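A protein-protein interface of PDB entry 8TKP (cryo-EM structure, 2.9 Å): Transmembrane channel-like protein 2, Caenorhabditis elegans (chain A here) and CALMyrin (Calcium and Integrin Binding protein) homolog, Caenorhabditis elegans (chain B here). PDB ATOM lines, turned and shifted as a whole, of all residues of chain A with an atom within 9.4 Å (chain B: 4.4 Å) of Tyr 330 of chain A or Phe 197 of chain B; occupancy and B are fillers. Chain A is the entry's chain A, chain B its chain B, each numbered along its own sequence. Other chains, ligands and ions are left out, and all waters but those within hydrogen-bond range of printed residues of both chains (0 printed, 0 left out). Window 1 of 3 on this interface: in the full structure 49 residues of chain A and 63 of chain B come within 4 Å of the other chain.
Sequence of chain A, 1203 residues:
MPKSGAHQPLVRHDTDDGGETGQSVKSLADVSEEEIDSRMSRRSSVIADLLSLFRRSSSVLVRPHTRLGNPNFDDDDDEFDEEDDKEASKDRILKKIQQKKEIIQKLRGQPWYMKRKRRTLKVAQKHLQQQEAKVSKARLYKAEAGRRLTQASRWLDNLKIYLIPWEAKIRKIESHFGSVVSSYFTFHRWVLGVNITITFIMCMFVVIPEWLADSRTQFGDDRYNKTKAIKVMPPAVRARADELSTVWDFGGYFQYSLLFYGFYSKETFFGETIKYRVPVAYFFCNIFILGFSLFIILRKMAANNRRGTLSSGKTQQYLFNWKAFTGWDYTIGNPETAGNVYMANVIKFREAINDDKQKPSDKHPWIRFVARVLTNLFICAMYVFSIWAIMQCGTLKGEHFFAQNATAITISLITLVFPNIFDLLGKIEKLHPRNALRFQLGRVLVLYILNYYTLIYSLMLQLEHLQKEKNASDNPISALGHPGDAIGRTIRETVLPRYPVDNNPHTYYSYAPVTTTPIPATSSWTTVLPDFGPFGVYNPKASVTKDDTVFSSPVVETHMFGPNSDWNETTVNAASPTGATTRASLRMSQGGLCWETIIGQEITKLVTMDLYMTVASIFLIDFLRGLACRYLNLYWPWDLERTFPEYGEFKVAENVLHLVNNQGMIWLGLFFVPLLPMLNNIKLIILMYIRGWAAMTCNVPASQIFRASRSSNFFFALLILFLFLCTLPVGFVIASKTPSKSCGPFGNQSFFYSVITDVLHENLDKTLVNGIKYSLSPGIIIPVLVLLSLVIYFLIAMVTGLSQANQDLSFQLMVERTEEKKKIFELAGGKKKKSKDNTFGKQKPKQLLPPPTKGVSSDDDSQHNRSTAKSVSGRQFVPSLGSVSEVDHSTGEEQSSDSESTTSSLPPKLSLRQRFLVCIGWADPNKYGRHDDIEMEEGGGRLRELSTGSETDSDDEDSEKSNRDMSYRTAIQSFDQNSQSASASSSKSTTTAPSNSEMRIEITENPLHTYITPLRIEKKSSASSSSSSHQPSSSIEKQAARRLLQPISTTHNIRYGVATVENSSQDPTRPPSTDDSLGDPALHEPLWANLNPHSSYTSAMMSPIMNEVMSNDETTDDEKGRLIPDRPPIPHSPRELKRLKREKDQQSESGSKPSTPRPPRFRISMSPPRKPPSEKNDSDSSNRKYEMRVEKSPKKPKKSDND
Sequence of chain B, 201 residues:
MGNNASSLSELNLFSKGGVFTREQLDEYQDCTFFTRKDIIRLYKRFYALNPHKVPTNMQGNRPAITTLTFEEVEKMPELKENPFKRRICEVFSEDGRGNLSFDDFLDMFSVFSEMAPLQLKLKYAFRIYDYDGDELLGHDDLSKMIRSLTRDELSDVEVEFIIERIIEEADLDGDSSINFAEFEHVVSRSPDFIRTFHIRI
Of the printed residues of chain B, Tyr 330 of chain A touches Asn 82, Phe 84, Ile 88, Phe 112, Tyr 129, Thr 196, Phe 197, His 198 and Ile 199. Phe 197 of chain B touches just one residue of chain A: Tyr 330 (3.8 Å). Thr 196 of chain B touches just these residues of chain A: Thr 326, Trp 328, Asp 329 and Tyr 330. Printed residues of chain B within 4 Å of Phe 325 of chain A: Tyr 129. Asn 334 of chain A touches none of the printed residues of chain B. The nearest residue of chain A that does not touch Phe 197 of chain B is Trp 328 of chain A (5.1 Å).
Hydrophobic or aromatic side chains of chain A within 4 Å of the printed part of chain B: Trp 328 and Tyr 330. Of the 15 printed residues of chain B, 11 touch a printed residue of chain A. Printed residues of chain B that touch a printed residue of chain A: Asn 82, Phe 84, Ile 88, Phe 112, Tyr 129, Phe 193, Arg 195, Thr 196, Phe 197, His 198 and Ile 199. Hydrophobic or aromatic side chains of chain B that line the printed part of chain A: Phe 84, Ile 88, Phe 112, Tyr 129, Phe 193, Phe 197, His 198 and Ile 199. Among the printed residues, no Asp or Glu carboxylate lies within 4 Å of a Lys or Arg side-chain nitrogen of the other chain.
The side-chain carboxylate (OD2) of Asp 329 of chain A lies within hydrogen-bond range of the side-chain hydroxyl (OG) of Ser 179 of chain A. The backbone NH (N) of Ile 199 of chain B sits at hydrogen-bond distance from the backbone carbonyl oxygen (O) of Phe 112 of chain B.
The side-chain hydroxyl (OG) of Ser 179 of chain A lies within hydrogen-bond range of the guanidinium group (NE) of Arg 195 of chain B (2.9 Å). The indole nitrogen of Trp 328 of chain A lies close to the side-chain amide nitrogen of Asn 82 of chain B (3.3 Å). The side-chain hydroxyl (OH) of Tyr 330 of chain A lies within hydrogen-bond range of the side-chain hydroxyl (OH) of Tyr 129 of chain B. The backbone NH (N) of Tyr 330 of chain A sits at hydrogen-bond distance from the backbone carbonyl oxygen (O) of Thr 196 of chain B. O of His 198 of chain B sits close to N of Thr 331 of chain A (3.4 Å). The backbone carbonyl oxygen (O) of Tyr 330 of chain A lies close to the backbone carbonyl oxygen (O) of His 198 of chain B (3.4 Å).
O of Trp 328 of chain A touches CB of Thr 196 of chain B, at 3.3 Å. Thr 196 of chain B touches Asp 329 of chain A (O to OD1, 3.6 Å). Asn 82 of chain B touches Tyr 330 of chain A (ND2 to CD2, 3.2 Å). CE1 of Phe 112 of chain B touches CD2 of Tyr 330 of chain A (3.7 Å).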
ATOM      1  N   ARG A 171      -3.104 -32.804 -17.159  1.00  0.00           N
ATOM      2  CA  ARG A 171      -4.202 -31.990 -16.652  1.00  0.00           C
ATOM      3  C   ARG A 171      -4.358 -32.147 -15.144  1.00  0.00           C
ATOM      4  O   ARG A 171      -4.557 -31.159 -14.430  1.00  0.00           O
ATOM      5  CB  ARG A 171      -5.501 -32.351 -17.369  1.00  0.00           C
ATOM      6  CG  ARG A 171      -6.716 -31.594 -16.858  1.00  0.00           C
ATOM      7  CD  ARG A 171      -7.921 -31.760 -17.771  1.00  0.00           C
ATOM      8  NE  ARG A 171      -8.332 -33.152 -17.915  1.00  0.00           N
ATOM      9  CZ  ARG A 171      -8.084 -33.900 -18.981  1.00  0.00           C
ATOM     10  NH1 ARG A 171      -7.427 -33.420 -20.024  1.00  0.00           N
ATOM     11  NH2 ARG A 171      -8.506 -35.161 -19.000  1.00  0.00           N
ATOM     12  N   GLU A 174      -1.422 -30.374 -13.428  1.00  0.00           N
ATOM     13  CA  GLU A 174      -1.621 -28.934 -13.510  1.00  0.00           C
ATOM     14  C   GLU A 174      -2.703 -28.469 -12.544  1.00  0.00           C
ATOM     15  O   GLU A 174      -2.558 -27.427 -11.894  1.00  0.00           O
ATOM     16  CB  GLU A 174      -1.977 -28.557 -14.946  1.00  0.00           C
ATOM     17  CG  GLU A 174      -2.318 -27.106 -15.166  1.00  0.00           C
ATOM     18  CD  GLU A 174      -2.589 -26.797 -16.624  1.00  0.00           C
ATOM     19  OE1 GLU A 174      -1.704 -27.068 -17.462  1.00  0.00           O
ATOM     20  OE2 GLU A 174      -3.689 -26.300 -16.937  1.00  0.00           O
ATOM     21  N   SER A 175      -3.794 -29.227 -12.439  1.00  0.00           N
ATOM     22  CA  SER A 175      -4.860 -28.869 -11.512  1.00  0.00           C
ATOM     23  C   SER A 175      -4.375 -28.918 -10.070  1.00  0.00           C
ATOM     24  O   SER A 175      -4.728 -28.054  -9.259  1.00  0.00           O
ATOM     25  CB  SER A 175      -6.057 -29.799 -11.708  1.00  0.00           C
ATOM     26  OG  SER A 175      -7.083 -29.513 -10.777  1.00  0.00           O
ATOM     27  N   PHE A 177      -1.159 -28.724  -8.887  1.00  0.00           N
ATOM     28  CA  PHE A 177      -0.044 -27.832  -8.588  1.00  0.00           C
ATOM     29  C   PHE A 177      -0.142 -26.500  -9.318  1.00  0.00           C
ATOM     30  O   PHE A 177      -0.135 -25.445  -8.677  1.00  0.00           O
ATOM     31  CB  PHE A 177       1.282 -28.523  -8.925  1.00  0.00           C
ATOM     32  CG  PHE A 177       1.672 -29.584  -7.947  1.00  0.00           C
ATOM     33  CD1 PHE A 177       2.246 -29.245  -6.735  1.00  0.00           C
ATOM     34  CD2 PHE A 177       1.463 -30.919  -8.233  1.00  0.00           C
ATOM     35  CE1 PHE A 177       2.604 -30.216  -5.828  1.00  0.00           C
ATOM     36  CE2 PHE A 177       1.820 -31.893  -7.331  1.00  0.00           C
ATOM     37  CZ  PHE A 177       2.392 -31.541  -6.125  1.00  0.00           C
ATOM     38  N   GLY A 178      -0.226 -26.511 -10.644  1.00  0.00           N
ATOM     39  CA  GLY A 178      -0.294 -25.263 -11.377  1.00  0.00           C
ATOM     40  C   GLY A 178       0.377 -25.301 -12.732  1.00  0.00           C
ATOM     41  O   GLY A 178       0.898 -26.338 -13.152  1.00  0.00           O
ATOM     42  N   SER A 179       0.369 -24.163 -13.426  1.00  0.00           N
ATOM     43  CA  SER A 179       0.945 -24.102 -14.762  1.00  0.00           C
ATOM     44  C   SER A 179       2.462 -24.225 -14.726  1.00  0.00           C
ATOM     45  O   SER A 179       3.061 -24.828 -15.623  1.00  0.00           O
ATOM     46  CB  SER A 179       0.529 -22.803 -15.449  1.00  0.00           C
ATOM     47  OG  SER A 179       0.895 -21.681 -14.666  1.00  0.00           O
ATOM     48  N   ALA A 324      -1.540  -7.623 -10.721  1.00  0.00           N
ATOM     49  CA  ALA A 324      -2.969  -7.626 -10.429  1.00  0.00           C
ATOM     50  C   ALA A 324      -3.785  -8.362 -11.484  1.00  0.00           C
ATOM     51  O   ALA A 324      -4.712  -9.100 -11.141  1.00  0.00           O
ATOM     52  CB  ALA A 324      -3.480  -6.192 -10.293  1.00  0.00           C
ATOM     53  N   PHE A 325      -3.463  -8.177 -12.761  1.00  0.00           N
ATOM     54  CA  PHE A 325      -4.221  -8.795 -13.842  1.00  0.00           C
ATOM     55  C   PHE A 325      -3.695 -10.170 -14.225  1.00  0.00           C
ATOM     56  O   PHE A 325      -4.301 -10.837 -15.068  1.00  0.00           O
ATOM     57  CB  PHE A 325      -4.228  -7.877 -15.065  1.00  0.00           C
ATOM     58  CG  PHE A 325      -4.963  -6.588 -14.844  1.00  0.00           C
ATOM     59  CD1 PHE A 325      -6.081  -6.549 -14.029  1.00  0.00           C
ATOM     60  CD2 PHE A 325      -4.531  -5.416 -15.436  1.00  0.00           C
ATOM     61  CE1 PHE A 325      -6.759  -5.366 -13.818  1.00  0.00           C
ATOM     62  CE2 PHE A 325      -5.206  -4.230 -15.227  1.00  0.00           C
ATOM     63  CZ  PHE A 325      -6.321  -4.206 -14.417  1.00  0.00           C
ATOM     64  N   THR A 326      -2.584 -10.606 -13.634  1.00  0.00           N
ATOM     65  CA  THR A 326      -2.095 -11.971 -13.778  1.00  0.00           C
ATOM     66  C   THR A 326      -1.851 -12.590 -12.408  1.00  0.00           C
ATOM     67  O   THR A 326      -1.046 -13.514 -12.267  1.00  0.00           O
ATOM     68  CB  THR A 326      -0.819 -12.023 -14.619  1.00  0.00           C
ATOM     69  OG1 THR A 326       0.240 -11.357 -13.923  1.00  0.00           O
ATOM     70  CG2 THR A 326      -1.035 -11.346 -15.964  1.00  0.00           C
ATOM     71  N   GLY A 327      -2.544 -12.086 -11.386  1.00  0.00           N
ATOM     72  CA  GLY A 327      -2.312 -12.510 -10.020  1.00  0.00           C
ATOM     73  C   GLY A 327      -2.931 -13.830  -9.630  1.00  0.00           C
ATOM     74  O   GLY A 327      -2.658 -14.321  -8.531  1.00  0.00           O
ATOM     75  N   TRP A 328      -3.757 -14.419 -10.491  1.00  0.00           N
ATOM     76  CA  TRP A 328      -4.365 -15.712 -10.213  1.00  0.00           C
ATOM     77  C   TRP A 328      -4.103 -16.665 -11.366  1.00  0.00           C
ATOM     78  O   TRP A 328      -4.171 -16.275 -12.535  1.00  0.00           O
ATOM     79  CB  TRP A 328      -5.872 -15.596  -9.981  1.00  0.00           C
ATOM     80  CG  TRP A 328      -6.485 -16.900  -9.590  1.00  0.00           C
ATOM     81  CD1 TRP A 328      -7.030 -17.831 -10.419  1.00  0.00           C
ATOM     82  CD2 TRP A 328      -6.597 -17.428  -8.265  1.00  0.00           C
ATOM     83  NE1 TRP A 328      -7.481 -18.906  -9.694  1.00  0.00           N
ATOM     84  CE2 TRP A 328      -7.226 -18.682  -8.366  1.00  0.00           C
ATOM     85  CE3 TRP A 328      -6.231 -16.957  -7.000  1.00  0.00           C
ATOM     86  CZ2 TRP A 328      -7.499 -19.472  -7.254  1.00  0.00           C
ATOM     87  CZ3 TRP A 328      -6.500 -17.743  -5.899  1.00  0.00           C
ATOM     88  CH2 TRP A 328      -7.129 -18.985  -6.032  1.00  0.00           C
ATOM     89  N   ASP A 329      -3.809 -17.916 -11.030  1.00  0.00           N
ATOM     90  CA  ASP A 329      -3.637 -18.976 -12.010  1.00  0.00           C
ATOM     91  C   ASP A 329      -4.964 -19.710 -12.155  1.00  0.00           C
ATOM     92  O   ASP A 329      -5.452 -20.313 -11.193  1.00  0.00           O
ATOM     93  CB  ASP A 329      -2.526 -19.937 -11.592  1.00  0.00           C
ATOM     94  CG  ASP A 329      -2.036 -20.803 -12.736  1.00  0.00           C
ATOM     95  OD1 ASP A 329      -2.814 -21.052 -13.679  1.00  0.00           O
ATOM     96  OD2 ASP A 329      -0.866 -21.236 -12.694  1.00  0.00           O
ATOM     97  N   TYR A 330      -5.540 -19.662 -13.355  1.00  0.00           N
ATOM     98  CA  TYR A 330      -6.825 -20.297 -13.609  1.00  0.00           C
ATOM     99  C   TYR A 330      -6.721 -21.810 -13.738  1.00  0.00           C
ATOM    100  O   TYR A 330      -7.754 -22.477 -13.853  1.00  0.00           O
ATOM    101  CB  TYR A 330      -7.459 -19.710 -14.873  1.00  0.00           C
ATOM    102  CG  TYR A 330      -8.011 -18.314 -14.688  1.00  0.00           C
ATOM    103  CD1 TYR A 330      -7.167 -17.223 -14.552  1.00  0.00           C
ATOM    104  CD2 TYR A 330      -9.380 -18.089 -14.658  1.00  0.00           C
ATOM    105  CE1 TYR A 330      -7.668 -15.948 -14.384  1.00  0.00           C
ATOM    106  CE2 TYR A 330      -9.890 -16.817 -14.490  1.00  0.00           C
ATOM    107  CZ  TYR A 330      -9.030 -15.752 -14.355  1.00  0.00           C
ATOM    108  OH  TYR A 330      -9.535 -14.484 -14.190  1.00  0.00           O
ATOM    109  N   THR A 331      -5.511 -22.359 -13.719  1.00  0.00           N
ATOM    110  CA  THR A 331      -5.299 -23.794 -13.842  1.00  0.00           C
ATOM    111  C   THR A 331      -5.344 -24.520 -12.504  1.00  0.00           C
ATOM    112  O   THR A 331      -5.171 -25.743 -12.475  1.00  0.00           O
ATOM    113  CB  THR A 331      -3.952 -24.066 -14.514  1.00  0.00           C
ATOM    114  OG1 THR A 331      -2.891 -23.671 -13.636  1.00  0.00           O
ATOM    115  CG2 THR A 331      -3.834 -23.289 -15.809  1.00  0.00           C
ATOM    116  N   ILE A 332      -5.569 -23.808 -11.406  1.00  0.00           N
ATOM    117  CA  ILE A 332      -5.538 -24.409 -10.078  1.00  0.00           C
ATOM    118  C   ILE A 332      -6.861 -25.110  -9.802  1.00  0.00           C
ATOM    119  O   ILE A 332      -7.938 -24.583 -10.103  1.00  0.00           O
ATOM    120  CB  ILE A 332      -5.244 -23.339  -9.012  1.00  0.00           C
ATOM    121  CG1 ILE A 332      -3.961 -22.587  -9.357  1.00  0.00           C
ATOM    122  CG2 ILE A 332      -5.133 -23.970  -7.638  1.00  0.00           C
ATOM    123  CD1 ILE A 332      -2.742 -23.468  -9.415  1.00  0.00           C
ATOM    124  N   GLY A 333      -6.782 -26.308  -9.228  1.00  0.00           N
ATOM    125  CA  GLY A 333      -7.971 -27.049  -8.855  1.00  0.00           C
ATOM    126  C   GLY A 333      -7.983 -27.477  -7.401  1.00  0.00           C
ATOM    127  O   GLY A 333      -9.029 -27.849  -6.865  1.00  0.00           O
ATOM    128  N   ASN A 334      -6.819 -27.432  -6.755  1.00  0.00           N
ATOM    129  CA  ASN A 334      -6.668 -27.841  -5.361  1.00  0.00           C
ATOM    130  C   ASN A 334      -6.852 -26.644  -4.434  1.00  0.00           C
ATOM    131  O   ASN A 334      -6.221 -25.602  -4.648  1.00  0.00           O
ATOM    132  CB  ASN A 334      -5.302 -28.465  -5.129  1.00  0.00           C
ATOM    133  CG  ASN A 334      -4.862 -28.377  -3.686  1.00  0.00           C
ATOM    134  OD1 ASN A 334      -4.039 -27.537  -3.328  1.00  0.00           O
ATOM    135  ND2 ASN A 334      -5.412 -29.244  -2.844  1.00  0.00           N
ATOM    136  N   VAL A 341      -1.716 -19.460  -3.250  1.00  0.00           N
ATOM    137  CA  VAL A 341      -1.727 -18.348  -4.200  1.00  0.00           C
ATOM    138  C   VAL A 341      -2.221 -17.075  -3.528  1.00  0.00           C
ATOM    139  O   VAL A 341      -1.692 -15.985  -3.769  1.00  0.00           O
ATOM    140  CB  VAL A 341      -2.574 -18.706  -5.436  1.00  0.00           C
ATOM    141  CG1 VAL A 341      -2.782 -17.482  -6.310  1.00  0.00           C
ATOM    142  CG2 VAL A 341      -1.901 -19.809  -6.235  1.00  0.00           C
ATOM    143  N   ASN B  82     -11.846 -21.136  -8.248  1.00  0.00           N
ATOM    144  CA  ASN B  82     -11.548 -19.862  -8.890  1.00  0.00           C
ATOM    145  C   ASN B  82     -12.346 -18.745  -8.227  1.00  0.00           C
ATOM    146  O   ASN B  82     -13.565 -18.867  -8.080  1.00  0.00           O
ATOM    147  CB  ASN B  82     -11.876 -19.927 -10.377  1.00  0.00           C
ATOM    148  CG  ASN B  82     -11.200 -18.831 -11.167  1.00  0.00           C
ATOM    149  OD1 ASN B  82     -11.714 -17.719 -11.275  1.00  0.00           O
ATOM    150  ND2 ASN B  82     -10.039 -19.140 -11.729  1.00  0.00           N
ATOM    151  N   PHE B  84     -13.201 -15.965  -9.448  1.00  0.00           N
ATOM    152  CA  PHE B  84     -14.044 -15.313 -10.436  1.00  0.00           C
ATOM    153  C   PHE B  84     -14.955 -16.286 -11.172  1.00  0.00           C
ATOM    154  O   PHE B  84     -15.368 -15.995 -12.297  1.00  0.00           O
ATOM    155  CB  PHE B  84     -13.181 -14.557 -11.446  1.00  0.00           C
ATOM    156  CG  PHE B  84     -12.103 -13.725 -10.819  1.00  0.00           C
ATOM    157  CD1 PHE B  84     -12.413 -12.549 -10.159  1.00  0.00           C
ATOM    158  CD2 PHE B  84     -10.778 -14.114 -10.897  1.00  0.00           C
ATOM    159  CE1 PHE B  84     -11.421 -11.780  -9.584  1.00  0.00           C
ATOM    160  CE2 PHE B  84      -9.782 -13.349 -10.325  1.00  0.00           C
ATOM    161  CZ  PHE B  84     -10.106 -12.181  -9.666  1.00  0.00           C
ATOM    162  N   ILE B  88     -17.019 -15.538 -14.511  1.00  0.00           N
ATOM    163  CA  ILE B  88     -16.872 -16.288 -15.756  1.00  0.00           C
ATOM    164  C   ILE B  88     -18.231 -16.777 -16.239  1.00  0.00           C
ATOM    165  O   ILE B  88     -18.581 -16.642 -17.420  1.00  0.00           O
ATOM    166  CB  ILE B  88     -15.890 -17.457 -15.563  1.00  0.00           C
ATOM    167  CG1 ILE B  88     -14.509 -16.932 -15.173  1.00  0.00           C
ATOM    168  CG2 ILE B  88     -15.793 -18.284 -16.828  1.00  0.00           C
ATOM    169  CD1 ILE B  88     -13.512 -18.021 -14.866  1.00  0.00           C
ATOM    170  N   PHE B 112     -10.707 -20.166 -22.822  1.00  0.00           N
ATOM    171  CA  PHE B 112      -9.659 -20.525 -21.875  1.00  0.00           C
ATOM    172  C   PHE B 112      -8.727 -21.606 -22.399  1.00  0.00           C
ATOM    173  O   PHE B 112      -7.795 -21.991 -21.686  1.00  0.00           O
ATOM    174  CB  PHE B 112     -10.278 -20.990 -20.556  1.00  0.00           C
ATOM    175  CG  PHE B 112     -10.855 -19.879 -19.731  1.00  0.00           C
ATOM    176  CD1 PHE B 112     -10.033 -19.064 -18.975  1.00  0.00           C
ATOM    177  CD2 PHE B 112     -12.217 -19.657 -19.700  1.00  0.00           C
ATOM    178  CE1 PHE B 112     -10.560 -18.048 -18.212  1.00  0.00           C
ATOM    179  CE2 PHE B 112     -12.749 -18.640 -18.940  1.00  0.00           C
ATOM    180  CZ  PHE B 112     -11.921 -17.833 -18.195  1.00  0.00           C
ATOM    181  N   LYS B 121      -8.495 -13.833 -25.560  1.00  0.00           N
ATOM    182  CA  LYS B 121      -8.372 -14.026 -24.122  1.00  0.00           C
ATOM    183  C   LYS B 121      -8.321 -12.689 -23.398  1.00  0.00           C
ATOM    184  O   LYS B 121      -8.901 -12.541 -22.320  1.00  0.00           O
ATOM    185  CB  LYS B 121      -7.134 -14.865 -23.808  1.00  0.00           C
ATOM    186  CG  LYS B 121      -7.021 -16.113 -24.661  1.00  0.00           C
ATOM    187  CD  LYS B 121      -5.825 -16.964 -24.276  1.00  0.00           C
ATOM    188  CE  LYS B 121      -6.214 -18.017 -23.259  1.00  0.00           C
ATOM    189  NZ  LYS B 121      -5.089 -18.939 -22.954  1.00  0.00           N
ATOM    190  N   ALA B 125     -11.009 -11.547 -20.672  1.00  0.00           N
ATOM    191  CA  ALA B 125     -10.523 -11.192 -19.342  1.00  0.00           C
ATOM    192  C   ALA B 125     -10.977  -9.793 -18.952  1.00  0.00           C
ATOM    193  O   ALA B 125     -11.370  -9.557 -17.803  1.00  0.00           O
ATOM    194  CB  ALA B 125      -9.000 -11.297 -19.295  1.00  0.00           C
ATOM    195  N   ILE B 128     -14.521 -10.090 -18.001  1.00  0.00           N
ATOM    196  CA  ILE B 128     -14.663 -10.721 -16.691  1.00  0.00           C
ATOM    197  C   ILE B 128     -14.411  -9.708 -15.583  1.00  0.00           C
ATOM    198  O   ILE B 128     -15.206  -9.572 -14.646  1.00  0.00           O
ATOM    199  CB  ILE B 128     -13.715 -11.927 -16.569  1.00  0.00           C
ATOM    200  CG1 ILE B 128     -14.214 -13.096 -17.415  1.00  0.00           C
ATOM    201  CG2 ILE B 128     -13.564 -12.345 -15.118  1.00  0.00           C
ATOM    202  CD1 ILE B 128     -13.269 -14.272 -17.433  1.00  0.00           C
ATOM    203  N   TYR B 129     -13.299  -8.977 -15.675  1.00  0.00           N
ATOM    204  CA  TYR B 129     -12.940  -8.039 -14.622  1.00  0.00           C
ATOM    205  C   TYR B 129     -13.830  -6.804 -14.603  1.00  0.00           C
ATOM    206  O   TYR B 129     -13.757  -6.027 -13.645  1.00  0.00           O
ATOM    207  CB  TYR B 129     -11.474  -7.630 -14.766  1.00  0.00           C
ATOM    208  CG  TYR B 129     -10.516  -8.796 -14.680  1.00  0.00           C
ATOM    209  CD1 TYR B 129     -10.812  -9.904 -13.899  1.00  0.00           C
ATOM    210  CD2 TYR B 129      -9.323  -8.796 -15.387  1.00  0.00           C
ATOM    211  CE1 TYR B 129      -9.947 -10.974 -13.821  1.00  0.00           C
ATOM    212  CE2 TYR B 129      -8.449  -9.864 -15.315  1.00  0.00           C
ATOM    213  CZ  TYR B 129      -8.768 -10.950 -14.529  1.00  0.00           C
ATOM    214  OH  TYR B 129      -7.904 -12.017 -14.451  1.00  0.00           O
ATOM    215  N   PHE B 193       0.306 -13.584 -18.598  1.00  0.00           N
ATOM    216  CA  PHE B 193      -1.126 -13.635 -18.875  1.00  0.00           C
ATOM    217  C   PHE B 193      -1.499 -14.892 -19.649  1.00  0.00           C
ATOM    218  O   PHE B 193      -2.520 -15.526 -19.358  1.00  0.00           O
ATOM    219  CB  PHE B 193      -1.564 -12.389 -19.640  1.00  0.00           C
ATOM    220  CG  PHE B 193      -3.018 -12.396 -20.016  1.00  0.00           C
ATOM    221  CD1 PHE B 193      -3.983 -12.014 -19.102  1.00  0.00           C
ATOM    222  CD2 PHE B 193      -3.418 -12.791 -21.281  1.00  0.00           C
ATOM    223  CE1 PHE B 193      -5.321 -12.023 -19.444  1.00  0.00           C
ATOM    224  CE2 PHE B 193      -4.753 -12.802 -21.627  1.00  0.00           C
ATOM    225  CZ  PHE B 193      -5.705 -12.416 -20.709  1.00  0.00           C
ATOM    226  N   ILE B 194      -0.691 -15.265 -20.642  1.00  0.00           N
ATOM    227  CA  ILE B 194      -0.979 -16.466 -21.420  1.00  0.00           C
ATOM    228  C   ILE B 194      -0.949 -17.698 -20.526  1.00  0.00           C
ATOM    229  O   ILE B 194      -1.808 -18.584 -20.634  1.00  0.00           O
ATOM    230  CB  ILE B 194       0.012 -16.590 -22.593  1.00  0.00           C
ATOM    231  CG1 ILE B 194      -0.295 -15.539 -23.660  1.00  0.00           C
ATOM    232  CG2 ILE B 194      -0.038 -17.985 -23.194  1.00  0.00           C
ATOM    233  CD1 ILE B 194      -1.611 -15.760 -24.367  1.00  0.00           C
ATOM    234  N   ARG B 195       0.033 -17.776 -19.629  1.00  0.00           N
ATOM    235  CA  ARG B 195       0.157 -18.942 -18.762  1.00  0.00           C
ATOM    236  C   ARG B 195      -0.980 -19.002 -17.746  1.00  0.00           C
ATOM    237  O   ARG B 195      -1.613 -20.048 -17.571  1.00  0.00           O
ATOM    238  CB  ARG B 195       1.513 -18.921 -18.055  1.00  0.00           C
ATOM    239  CG  ARG B 195       1.966 -20.275 -17.541  1.00  0.00           C
ATOM    240  CD  ARG B 195       3.168 -20.154 -16.615  1.00  0.00           C
ATOM    241  NE  ARG B 195       2.803 -19.617 -15.308  1.00  0.00           N
ATOM    242  CZ  ARG B 195       2.952 -18.350 -14.950  1.00  0.00           C
ATOM    243  NH1 ARG B 195       3.467 -17.453 -15.774  1.00  0.00           N
ATOM    244  NH2 ARG B 195       2.577 -17.973 -13.730  1.00  0.00           N
ATOM    245  N   THR B 196      -1.250 -17.887 -17.063  1.00  0.00           N
ATOM    246  CA  THR B 196      -2.246 -17.896 -15.997  1.00  0.00           C
ATOM    247  C   THR B 196      -3.660 -18.036 -16.550  1.00  0.00           C
ATOM    248  O   THR B 196      -4.446 -18.860 -16.071  1.00  0.00           O
ATOM    249  CB  THR B 196      -2.129 -16.626 -15.155  1.00  0.00           C
ATOM    250  OG1 THR B 196      -2.314 -15.477 -15.992  1.00  0.00           O
ATOM    251  CG2 THR B 196      -0.763 -16.551 -14.494  1.00  0.00           C
ATOM    252  N   PHE B 197      -4.003 -17.239 -17.563  1.00  0.00           N
ATOM    253  CA  PHE B 197      -5.356 -17.232 -18.119  1.00  0.00           C
ATOM    254  C   PHE B 197      -5.518 -18.466 -18.999  1.00  0.00           C
ATOM    255  O   PHE B 197      -5.471 -18.410 -20.229  1.00  0.00           O
ATOM    256  CB  PHE B 197      -5.609 -15.947 -18.897  1.00  0.00           C
ATOM    257  CG  PHE B 197      -7.061 -15.625 -19.086  1.00  0.00           C
ATOM    258  CD1 PHE B 197      -7.787 -15.026 -18.073  1.00  0.00           C
ATOM    259  CD2 PHE B 197      -7.697 -15.910 -20.280  1.00  0.00           C
ATOM    260  CE1 PHE B 197      -9.121 -14.723 -18.243  1.00  0.00           C
ATOM    261  CE2 PHE B 197      -9.034 -15.611 -20.455  1.00  0.00           C
ATOM    262  CZ  PHE B 197      -9.746 -15.015 -19.436  1.00  0.00           C
ATOM    263  N   HIS B 198      -5.710 -19.608 -18.346  1.00  0.00           N
ATOM    264  CA  HIS B 198      -5.781 -20.885 -19.039  1.00  0.00           C
ATOM    265  C   HIS B 198      -6.575 -21.864 -18.187  1.00  0.00           C
ATOM    266  O   HIS B 198      -6.404 -21.909 -16.967  1.00  0.00           O
ATOM    267  CB  HIS B 198      -4.378 -21.434 -19.319  1.00  0.00           C
ATOM    268  CG  HIS B 198      -4.366 -22.685 -20.137  1.00  0.00           C
ATOM    269  ND1 HIS B 198      -4.710 -23.917 -19.622  1.00  0.00           N
ATOM    270  CD2 HIS B 198      -4.035 -22.900 -21.431  1.00  0.00           C
ATOM    271  CE1 HIS B 198      -4.600 -24.833 -20.566  1.00  0.00           C
ATOM    272  NE2 HIS B 198      -4.192 -24.243 -21.674  1.00  0.00           N
ATOM    273  N   ILE B 199      -7.452 -22.630 -18.831  1.00  0.00           N
ATOM    274  CA  ILE B 199      -8.191 -23.685 -18.146  1.00  0.00           C
ATOM    275  C   ILE B 199      -8.167 -24.939 -19.007  1.00  0.00           C
ATOM    276  O   ILE B 199      -8.932 -25.061 -19.970  1.00  0.00           O
ATOM    277  CB  ILE B 199      -9.638 -23.261 -17.830  1.00  0.00           C
ATOM    278  CG1 ILE B 199      -9.654 -22.072 -16.869  1.00  0.00           C
ATOM    279  CG2 ILE B 199     -10.412 -24.424 -17.233  1.00  0.00           C
ATOM    280  CD1 ILE B 199     -11.040 -21.648 -16.449  1.00  0.00           C
